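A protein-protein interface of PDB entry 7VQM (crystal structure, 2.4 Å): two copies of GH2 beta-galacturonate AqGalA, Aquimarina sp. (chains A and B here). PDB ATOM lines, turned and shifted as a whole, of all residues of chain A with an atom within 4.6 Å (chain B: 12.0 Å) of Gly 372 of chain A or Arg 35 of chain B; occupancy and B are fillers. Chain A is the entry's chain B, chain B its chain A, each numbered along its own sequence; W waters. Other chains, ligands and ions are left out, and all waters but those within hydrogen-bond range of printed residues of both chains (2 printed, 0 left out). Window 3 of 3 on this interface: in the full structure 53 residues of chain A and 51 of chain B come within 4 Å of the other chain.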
ATOM      1  N   ASN A 172     -16.997 -16.913  18.396  1.00  0.00           N
ATOM      2  CA  ASN A 172     -16.428 -18.271  18.158  1.00  0.00           C
ATOM      3  C   ASN A 172     -15.178 -18.192  17.250  1.00  0.00           C
ATOM      4  O   ASN A 172     -14.184 -17.574  17.689  1.00  0.00           O
ATOM      5  CB  ASN A 172     -17.527 -19.264  17.758  1.00  0.00           C
ATOM      6  CG  ASN A 172     -18.413 -18.852  16.601  1.00  0.00           C
ATOM      7  OD1 ASN A 172     -18.360 -17.740  16.090  1.00  0.00           O
ATOM      8  ND2 ASN A 172     -19.244 -19.776  16.176  1.00  0.00           N
ATOM      9  N   TYR A 370     -21.559 -12.037  16.436  1.00  0.00           N
ATOM     10  CA  TYR A 370     -20.794 -11.531  15.272  1.00  0.00           C
ATOM     11  C   TYR A 370     -20.531 -12.638  14.270  1.00  0.00           C
ATOM     12  O   TYR A 370     -19.798 -13.581  14.610  1.00  0.00           O
ATOM     13  CB  TYR A 370     -19.497 -10.982  15.861  1.00  0.00           C
ATOM     14  CG  TYR A 370     -18.527 -10.281  14.952  1.00  0.00           C
ATOM     15  CD1 TYR A 370     -17.642 -10.999  14.163  1.00  0.00           C
ATOM     16  CD2 TYR A 370     -18.423  -8.901  14.957  1.00  0.00           C
ATOM     17  CE1 TYR A 370     -16.717 -10.360  13.360  1.00  0.00           C
ATOM     18  CE2 TYR A 370     -17.501  -8.250  14.160  1.00  0.00           C
ATOM     19  CZ  TYR A 370     -16.650  -8.983  13.356  1.00  0.00           C
ATOM     20  OH  TYR A 370     -15.739  -8.357  12.570  1.00  0.00           O
ATOM     21  N   TRP A 371     -21.131 -12.517  13.084  1.00  0.00           N
ATOM     22  CA  TRP A 371     -20.934 -13.503  11.985  1.00  0.00           C
ATOM     23  C   TRP A 371     -21.575 -14.852  12.317  1.00  0.00           C
ATOM     24  O   TRP A 371     -22.739 -14.849  12.716  1.00  0.00           O
ATOM     25  CB  TRP A 371     -19.446 -13.670  11.651  1.00  0.00           C
ATOM     26  CG  TRP A 371     -18.795 -12.464  11.043  1.00  0.00           C
ATOM     27  CD1 TRP A 371     -19.411 -11.364  10.515  1.00  0.00           C
ATOM     28  CD2 TRP A 371     -17.381 -12.244  10.884  1.00  0.00           C
ATOM     29  NE1 TRP A 371     -18.480 -10.477  10.053  1.00  0.00           N
ATOM     30  CE2 TRP A 371     -17.226 -10.987  10.262  1.00  0.00           C
ATOM     31  CE3 TRP A 371     -16.237 -12.975  11.217  1.00  0.00           C
ATOM     32  CZ2 TRP A 371     -15.973 -10.450   9.967  1.00  0.00           C
ATOM     33  CZ3 TRP A 371     -14.999 -12.448  10.925  1.00  0.00           C
ATOM     34  CH2 TRP A 371     -14.870 -11.202  10.309  1.00  0.00           C
ATOM     35  N   GLY A 372     -20.818 -15.946  12.190  1.00  0.00           N
ATOM     36  CA  GLY A 372     -21.365 -17.307  12.308  1.00  0.00           C
ATOM     37  C   GLY A 372     -21.412 -17.914  13.700  1.00  0.00           C
ATOM     38  O   GLY A 372     -20.896 -19.026  13.863  1.00  0.00           O
ATOM     39  N   ILE A 373     -21.987 -17.219  14.669  1.00  0.00           N
ATOM     40  CA  ILE A 373     -22.363 -17.792  15.987  1.00  0.00           C
ATOM     41  C   ILE A 373     -23.245 -19.019  15.754  1.00  0.00           C
ATOM     42  O   ILE A 373     -24.066 -18.964  14.828  1.00  0.00           O
ATOM     43  CB  ILE A 373     -23.110 -16.724  16.812  1.00  0.00           C
ATOM     44  CG1 ILE A 373     -22.209 -15.535  17.148  1.00  0.00           C
ATOM     45  CG2 ILE A 373     -23.764 -17.320  18.057  1.00  0.00           C
ATOM     46  CD1 ILE A 373     -20.950 -15.887  17.921  1.00  0.00           C
ATOM     47  N   ASP A 374     -23.106 -20.055  16.585  1.00  0.00           N
ATOM     48  CA  ASP A 374     -23.909 -21.308  16.525  1.00  0.00           C
ATOM     49  C   ASP A 374     -25.298 -21.028  17.127  1.00  0.00           C
ATOM     50  O   ASP A 374     -25.467 -21.302  18.341  1.00  0.00           O
ATOM     51  CB  ASP A 374     -23.155 -22.442  17.232  1.00  0.00           C
ATOM     52  CG  ASP A 374     -23.565 -23.854  16.837  1.00  0.00           C
ATOM     53  OD1 ASP A 374     -24.439 -23.996  15.970  1.00  0.00           O
ATOM     54  OD2 ASP A 374     -23.011 -24.807  17.410  1.00  0.00           O
ATOM     55  N   GLU A 409     -23.813  -7.928  11.825  1.00  0.00           N
ATOM     56  CA  GLU A 409     -23.599  -8.789  10.619  1.00  0.00           C
ATOM     57  C   GLU A 409     -23.919 -10.253  10.917  1.00  0.00           C
ATOM     58  O   GLU A 409     -22.990 -11.027  11.092  1.00  0.00           O
ATOM     59  CB  GLU A 409     -22.182  -8.603  10.066  1.00  0.00           C
ATOM     60  CG  GLU A 409     -21.938  -7.206   9.530  1.00  0.00           C
ATOM     61  CD  GLU A 409     -20.497  -6.881   9.192  1.00  0.00           C
ATOM     62  OE1 GLU A 409     -19.676  -7.805   9.152  1.00  0.00           O
ATOM     63  OE2 GLU A 409     -20.202  -5.697   8.966  1.00  0.00           O
ATOM     64  N   THR A 410     -25.197 -10.607  10.899  1.00  0.00           N
ATOM     65  CA  THR A 410     -25.664 -11.975  11.213  1.00  0.00           C
ATOM     66  C   THR A 410     -26.411 -12.562  10.021  1.00  0.00           C
ATOM     67  O   THR A 410     -27.145 -11.827   9.375  1.00  0.00           O
ATOM     68  CB  THR A 410     -26.556 -11.944  12.455  1.00  0.00           C
ATOM     69  OG1 THR A 410     -27.707 -11.136  12.212  1.00  0.00           O
ATOM     70  CG2 THR A 410     -25.815 -11.430  13.671  1.00  0.00           C
ATOM     71  N   PRO A 411     -26.290 -13.881   9.727  1.00  0.00           N
ATOM     72  CA  PRO A 411     -26.945 -14.482   8.563  1.00  0.00           C
ATOM     73  C   PRO A 411     -28.471 -14.432   8.671  1.00  0.00           C
ATOM     74  O   PRO A 411     -28.951 -14.532   9.768  1.00  0.00           O
ATOM     75  CB  PRO A 411     -26.496 -15.946   8.615  1.00  0.00           C
ATOM     76  CG  PRO A 411     -26.215 -16.172  10.077  1.00  0.00           C
ATOM     77  CD  PRO A 411     -25.561 -14.882  10.521  1.00  0.00           C
ATOM     78  N   GLU A 441     -27.143  -5.427   7.298  1.00  0.00           N
ATOM     79  CA  GLU A 441     -26.518  -5.351   5.955  1.00  0.00           C
ATOM     80  C   GLU A 441     -27.620  -5.137   4.905  1.00  0.00           C
ATOM     81  O   GLU A 441     -28.814  -5.447   5.193  1.00  0.00           O
ATOM     82  CB  GLU A 441     -25.686  -6.618   5.760  1.00  0.00           C
ATOM     83  CG  GLU A 441     -24.484  -6.680   6.688  1.00  0.00           C
ATOM     84  CD  GLU A 441     -23.895  -8.068   6.795  1.00  0.00           C
ATOM     85  OE1 GLU A 441     -24.571  -8.950   7.370  1.00  0.00           O
ATOM     86  OE2 GLU A 441     -22.782  -8.269   6.288  1.00  0.00           O
ATOM     87  N   TYR B  27      -7.185 -17.266  12.411  1.00  0.00           N
ATOM     88  CA  TYR B  27      -8.639 -17.309  12.137  1.00  0.00           C
ATOM     89  C   TYR B  27      -8.896 -17.903  10.748  1.00  0.00           C
ATOM     90  O   TYR B  27     -10.029 -17.761  10.225  1.00  0.00           O
ATOM     91  CB  TYR B  27      -9.234 -15.908  12.223  1.00  0.00           C
ATOM     92  CG  TYR B  27      -9.161 -15.226  13.564  1.00  0.00           C
ATOM     93  CD1 TYR B  27      -8.531 -15.786  14.671  1.00  0.00           C
ATOM     94  CD2 TYR B  27      -9.730 -13.972  13.716  1.00  0.00           C
ATOM     95  CE1 TYR B  27      -8.489 -15.120  15.888  1.00  0.00           C
ATOM     96  CE2 TYR B  27      -9.700 -13.303  14.925  1.00  0.00           C
ATOM     97  CZ  TYR B  27      -9.067 -13.868  16.009  1.00  0.00           C
ATOM     98  OH  TYR B  27      -9.054 -13.154  17.172  1.00  0.00           O
ATOM     99  N   GLU B  28      -7.872 -18.523  10.154  1.00  0.00           N
ATOM    100  CA  GLU B  28      -7.961 -19.250   8.851  1.00  0.00           C
ATOM    101  C   GLU B  28      -8.536 -18.332   7.759  1.00  0.00           C
ATOM    102  O   GLU B  28      -9.147 -18.842   6.839  1.00  0.00           O
ATOM    103  CB  GLU B  28      -8.777 -20.535   9.029  1.00  0.00           C
ATOM    104  CG  GLU B  28      -8.311 -21.363  10.211  1.00  0.00           C
ATOM    105  CD  GLU B  28      -8.688 -22.834  10.193  1.00  0.00           C
ATOM    106  OE1 GLU B  28      -8.993 -23.341   9.097  1.00  0.00           O
ATOM    107  OE2 GLU B  28      -8.620 -23.486  11.277  1.00  0.00           O
ATOM    108  N   THR B  29      -8.266 -17.029   7.836  1.00  0.00           N
ATOM    109  CA  THR B  29      -8.747 -15.968   6.905  1.00  0.00           C
ATOM    110  C   THR B  29      -8.482 -16.380   5.453  1.00  0.00           C
ATOM    111  O   THR B  29      -9.389 -16.198   4.624  1.00  0.00           O
ATOM    112  CB  THR B  29      -8.073 -14.626   7.210  1.00  0.00           C
ATOM    113  OG1 THR B  29      -8.287 -14.316   8.588  1.00  0.00           O
ATOM    114  CG2 THR B  29      -8.584 -13.496   6.344  1.00  0.00           C
ATOM    115  N   GLY B  30      -7.306 -16.952   5.179  1.00  0.00           N
ATOM    116  CA  GLY B  30      -6.849 -17.302   3.824  1.00  0.00           C
ATOM    117  C   GLY B  30      -7.456 -18.581   3.273  1.00  0.00           C
ATOM    118  O   GLY B  30      -7.385 -18.770   2.044  1.00  0.00           O
ATOM    119  N   TYR B  31      -8.024 -19.430   4.136  1.00  0.00           N
ATOM    120  CA  TYR B  31      -8.439 -20.829   3.850  1.00  0.00           C
ATOM    121  C   TYR B  31      -9.970 -20.985   3.871  1.00  0.00           C
ATOM    122  O   TYR B  31     -10.532 -21.779   3.090  1.00  0.00           O
ATOM    123  CB  TYR B  31      -7.811 -21.745   4.903  1.00  0.00           C
ATOM    124  CG  TYR B  31      -8.070 -23.215   4.698  1.00  0.00           C
ATOM    125  CD1 TYR B  31      -7.606 -23.864   3.572  1.00  0.00           C
ATOM    126  CD2 TYR B  31      -8.752 -23.969   5.633  1.00  0.00           C
ATOM    127  CE1 TYR B  31      -7.837 -25.212   3.363  1.00  0.00           C
ATOM    128  CE2 TYR B  31      -8.992 -25.322   5.442  1.00  0.00           C
ATOM    129  CZ  TYR B  31      -8.535 -25.950   4.299  1.00  0.00           C
ATOM    130  OH  TYR B  31      -8.755 -27.281   4.074  1.00  0.00           O
ATOM    131  N   ARG B  32     -10.659 -20.294   4.781  1.00  0.00           N
ATOM    132  CA  ARG B  32     -12.118 -20.498   4.988  1.00  0.00           C
ATOM    133  C   ARG B  32     -12.886 -19.190   4.831  1.00  0.00           C
ATOM    134  O   ARG B  32     -12.368 -18.142   5.246  1.00  0.00           O
ATOM    135  CB  ARG B  32     -12.401 -21.010   6.397  1.00  0.00           C
ATOM    136  CG  ARG B  32     -11.872 -22.403   6.668  1.00  0.00           C
ATOM    137  CD  ARG B  32     -12.274 -22.783   8.074  1.00  0.00           C
ATOM    138  NE  ARG B  32     -11.637 -24.027   8.432  1.00  0.00           N
ATOM    139  CZ  ARG B  32     -12.165 -25.242   8.318  1.00  0.00           C
ATOM    140  NH1 ARG B  32     -13.402 -25.449   7.874  1.00  0.00           N
ATOM    141  NH2 ARG B  32     -11.406 -26.266   8.669  1.00  0.00           N
ATOM    142  N   ASN B  33     -14.119 -19.286   4.346  1.00  0.00           N
ATOM    143  CA  ASN B  33     -15.089 -18.162   4.324  1.00  0.00           C
ATOM    144  C   ASN B  33     -15.360 -17.758   5.776  1.00  0.00           C
ATOM    145  O   ASN B  33     -15.784 -18.614   6.566  1.00  0.00           O
ATOM    146  CB  ASN B  33     -16.328 -18.562   3.521  1.00  0.00           C
ATOM    147  CG  ASN B  33     -17.439 -17.533   3.513  1.00  0.00           C
ATOM    148  OD1 ASN B  33     -17.976 -17.172   4.551  1.00  0.00           O
ATOM    149  ND2 ASN B  33     -17.842 -17.103   2.330  1.00  0.00           N
ATOM    150  N   HIS B  34     -15.100 -16.495   6.120  1.00  0.00           N
ATOM    151  CA  HIS B  34     -15.232 -15.964   7.507  1.00  0.00           C
ATOM    152  C   HIS B  34     -16.695 -15.973   8.001  1.00  0.00           C
ATOM    153  O   HIS B  34     -16.881 -15.807   9.205  1.00  0.00           O
ATOM    154  CB  HIS B  34     -14.577 -14.584   7.595  1.00  0.00           C
ATOM    155  CG  HIS B  34     -15.272 -13.542   6.794  1.00  0.00           C
ATOM    156  ND1 HIS B  34     -15.125 -13.448   5.428  1.00  0.00           N
ATOM    157  CD2 HIS B  34     -16.118 -12.553   7.160  1.00  0.00           C
ATOM    158  CE1 HIS B  34     -15.847 -12.438   4.984  1.00  0.00           C
ATOM    159  NE2 HIS B  34     -16.484 -11.885   6.025  1.00  0.00           N
ATOM    160  N   ARG B  35     -17.696 -16.178   7.132  1.00  0.00           N
ATOM    161  CA  ARG B  35     -19.143 -16.132   7.501  1.00  0.00           C
ATOM    162  C   ARG B  35     -19.690 -17.540   7.780  1.00  0.00           C
ATOM    163  O   ARG B  35     -20.469 -17.681   8.724  1.00  0.00           O
ATOM    164  CB  ARG B  35     -19.990 -15.449   6.420  1.00  0.00           C
ATOM    165  CG  ARG B  35     -19.587 -14.018   6.089  1.00  0.00           C
ATOM    166  CD  ARG B  35     -19.636 -13.035   7.250  1.00  0.00           C
ATOM    167  NE  ARG B  35     -20.998 -12.792   7.716  1.00  0.00           N
ATOM    168  CZ  ARG B  35     -21.752 -11.726   7.424  1.00  0.00           C
ATOM    169  NH1 ARG B  35     -21.290 -10.745   6.664  1.00  0.00           N
ATOM    170  NH2 ARG B  35     -22.981 -11.646   7.909  1.00  0.00           N
ATOM    171  N   ASN B  36     -19.323 -18.548   6.996  1.00  0.00           N
ATOM    172  CA  ASN B  36     -19.945 -19.900   7.095  1.00  0.00           C
ATOM    173  C   ASN B  36     -18.897 -20.963   7.471  1.00  0.00           C
ATOM    174  O   ASN B  36     -19.292 -22.116   7.633  1.00  0.00           O
ATOM    175  CB  ASN B  36     -20.660 -20.266   5.793  1.00  0.00           C
ATOM    176  CG  ASN B  36     -19.756 -20.193   4.573  1.00  0.00           C
ATOM    177  OD1 ASN B  36     -18.552 -20.464   4.644  1.00  0.00           O
ATOM    178  ND2 ASN B  36     -20.324 -19.835   3.431  1.00  0.00           N
ATOM    179  N   TRP B  37     -17.613 -20.590   7.520  1.00  0.00           N
ATOM    180  CA  TRP B  37     -16.458 -21.421   7.953  1.00  0.00           C
ATOM    181  C   TRP B  37     -16.111 -22.492   6.901  1.00  0.00           C
ATOM    182  O   TRP B  37     -15.217 -23.334   7.179  1.00  0.00           O
ATOM    183  CB  TRP B  37     -16.727 -22.022   9.346  1.00  0.00           C
ATOM    184  CG  TRP B  37     -15.490 -22.426  10.086  1.00  0.00           C
ATOM    185  CD1 TRP B  37     -15.188 -23.675  10.548  1.00  0.00           C
ATOM    186  CD2 TRP B  37     -14.383 -21.589  10.453  1.00  0.00           C
ATOM    187  NE1 TRP B  37     -13.981 -23.671  11.188  1.00  0.00           N
ATOM    188  CE2 TRP B  37     -13.459 -22.404  11.138  1.00  0.00           C
ATOM    189  CE3 TRP B  37     -14.070 -20.239  10.274  1.00  0.00           C
ATOM    190  CZ2 TRP B  37     -12.241 -21.910  11.607  1.00  0.00           C
ATOM    191  CZ3 TRP B  37     -12.877 -19.747  10.760  1.00  0.00           C
ATOM    192  CH2 TRP B  37     -11.973 -20.575  11.410  1.00  0.00           C
ATOM    193  N   ILE B  38     -16.723 -22.453   5.714  1.00  0.00           N
ATOM    194  CA  ILE B  38     -16.504 -23.486   4.651  1.00  0.00           C
ATOM    195  C   ILE B  38     -15.199 -23.174   3.923  1.00  0.00           C
ATOM    196  O   ILE B  38     -14.976 -22.024   3.541  1.00  0.00           O
ATOM    197  CB  ILE B  38     -17.706 -23.565   3.683  1.00  0.00           C
ATOM    198  CG1 ILE B  38     -18.907 -24.241   4.351  1.00  0.00           C
ATOM    199  CG2 ILE B  38     -17.329 -24.253   2.378  1.00  0.00           C
ATOM    200  CD1 ILE B  38     -20.182 -24.156   3.547  1.00  0.00           C
ATOM    201  N   PRO B  39     -14.307 -24.173   3.708  1.00  0.00           N
ATOM    202  CA  PRO B  39     -13.052 -23.935   3.006  1.00  0.00           C
ATOM    203  C   PRO B  39     -13.345 -23.467   1.571  1.00  0.00           C
ATOM    204  O   PRO B  39     -14.222 -24.042   0.913  1.00  0.00           O
ATOM    205  CB  PRO B  39     -12.320 -25.281   3.082  1.00  0.00           C
ATOM    206  CG  PRO B  39     -12.980 -25.999   4.266  1.00  0.00           C
ATOM    207  CD  PRO B  39     -14.425 -25.563   4.167  1.00  0.00           C
ATOM    208  N   PHE B  40     -12.657 -22.402   1.136  1.00  0.00           N
ATOM    209  CA  PHE B  40     -12.689 -21.895  -0.259  1.00  0.00           C
ATOM    210  C   PHE B  40     -12.477 -23.068  -1.223  1.00  0.00           C
ATOM    211  O   PHE B  40     -13.116 -23.072  -2.263  1.00  0.00           O
ATOM    212  CB  PHE B  40     -11.649 -20.784  -0.478  1.00  0.00           C
ATOM    213  CG  PHE B  40     -11.848 -19.528   0.341  1.00  0.00           C
ATOM    214  CD1 PHE B  40     -13.034 -18.810   0.278  1.00  0.00           C
ATOM    215  CD2 PHE B  40     -10.847 -19.055   1.170  1.00  0.00           C
ATOM    216  CE1 PHE B  40     -13.209 -17.651   1.019  1.00  0.00           C
ATOM    217  CE2 PHE B  40     -11.023 -17.895   1.906  1.00  0.00           C
ATOM    218  CZ  PHE B  40     -12.199 -17.190   1.827  1.00  0.00           C
ATOM    219  N   MET B  43     -15.681 -24.713  -2.689  1.00  0.00           N
ATOM    220  CA  MET B  43     -16.556 -23.752  -3.409  1.00  0.00           C
ATOM    221  C   MET B  43     -15.844 -23.309  -4.693  1.00  0.00           C
ATOM    222  O   MET B  43     -16.456 -23.469  -5.760  1.00  0.00           O
ATOM    223  CB  MET B  43     -16.838 -22.519  -2.545  1.00  0.00           C
ATOM    224  CG  MET B  43     -17.281 -22.832  -1.116  1.00  0.00           C
ATOM    225  SD  MET B  43     -17.178 -21.386   0.016  1.00  0.00           S
ATOM    226  CE  MET B  43     -18.705 -20.515  -0.343  1.00  0.00           C
ATOM    227  N   LYS B  51      -9.690 -13.769  -2.575  1.00  0.00           N
ATOM    228  CA  LYS B  51      -9.694 -14.038  -1.100  1.00  0.00           C
ATOM    229  C   LYS B  51      -8.728 -15.157  -0.695  1.00  0.00           C
ATOM    230  O   LYS B  51      -8.028 -15.022   0.313  1.00  0.00           O
ATOM    231  CB  LYS B  51     -11.108 -14.387  -0.623  1.00  0.00           C
ATOM    232  CG  LYS B  51     -12.008 -13.183  -0.365  1.00  0.00           C
ATOM    233  CD  LYS B  51     -13.403 -13.283  -0.961  1.00  0.00           C
ATOM    234  CE  LYS B  51     -14.515 -13.405   0.063  1.00  0.00           C
ATOM    235  NZ  LYS B  51     -15.844 -13.481  -0.599  1.00  0.00           N
HETATM  236  O   HOH W   1     -17.790 -10.019   6.784  1.00  0.00           O
HETATM  237  O   HOH W   2     -17.952 -16.783  11.371  1.00  0.00           O
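OE2 of Glu 441 of chain A is in salt-bridge range of NH1 of Arg 35 of chain B. NH2 of Arg 35 of chain B sits at hydrogen-bond distance from O of Glu 409 of chain A (3.2 Å).
No position is printed for both chains. Of the 6 pairs that touch across the chains among the printed residues, none has its exchanged pair printed and touching as well.
Among the printed residues, pairs that only touch across the chains: Trp 371 of chain A with His 34 of chain B, Trp 371 of chain A with Arg 35 of chain B, Gly 372 of chain A with Arg 35 of chain B and Thr 410 of chain A with Arg 35 of chain B.
Water W1 lies within hydrogen-bond range of NE2 of His 34 of chain B (2.4 Å) and NE1 of Trp 371 of chain A (3.4 Å). Water W2 bridges O of His 34 of chain B (2.6 Å) and N of Gly 372 of chain A (3.1 Å).
The backbone NH (N) of Arg 35 of chain B sits at hydrogen-bond distance from the side-chain amide oxygen (OD1) of Asn 33 of chain B, at 2.8 Å. The side-chain carboxylate (OE1) of Glu 409 of chain A is in hydrogen-bond range of the indole nitrogen (NE1) of Trp 371 of chain A. ND2 of Asn 172 of chain A is in hydrogen-bond range of O of Gly 372 of chain A (2.9 Å).
Arg 35 of chain B touches just these residues of chain A: Trp 371 (3.5 Å), Gly 372 (3.7 Å), Glu 409 (3.2 Å), Thr 410 (3.9 Å) and Glu 441 (2.9 Å). No residue of chain B comes within 4 Å of Asn 172 of chain A. Of the printed residues of chain B, Trp 371 of chain A touches His 34 and Arg 35. No residue of chain B comes within 4 Å of Ile 373 of chain A. Glu 409 of chain A touches just one residue of chain B: Arg 35 (3.2 Å). Thr 410 of chain A touches just one residue of chain B: Arg 35 (3.9 Å). No residue of chain B comes within 4 Å of Pro 411 of chain A. Printed residues of chain B within 4 Å of Glu 441 of chain A: Arg 35 (2.9 Å). Of the printed residues of chain A, His 34 of chain B touches Trp 371. Thr 29 of chain B touches none of the printed residues of chain A. Tyr 27 of chain B touches none of the printed residues of chain A.
Hydrophobic or aromatic side chains of chain A within 4 Å of the printed part of chain B: Trp 371. Along chain A the printed residues that touch a printed residue of chain B span positions 371 to 441. Printed residues of chain B that touch a printed residue of chain A: His 34 and Arg 35. Among the printed residues, 6 pairs touch across the chains. Among the printed residues, Asp or Glu carboxylates within 4 Å of a Lys or Arg side-chain nitrogen of the other chain: Glu 441 of chain A with Arg 35 of chain B.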
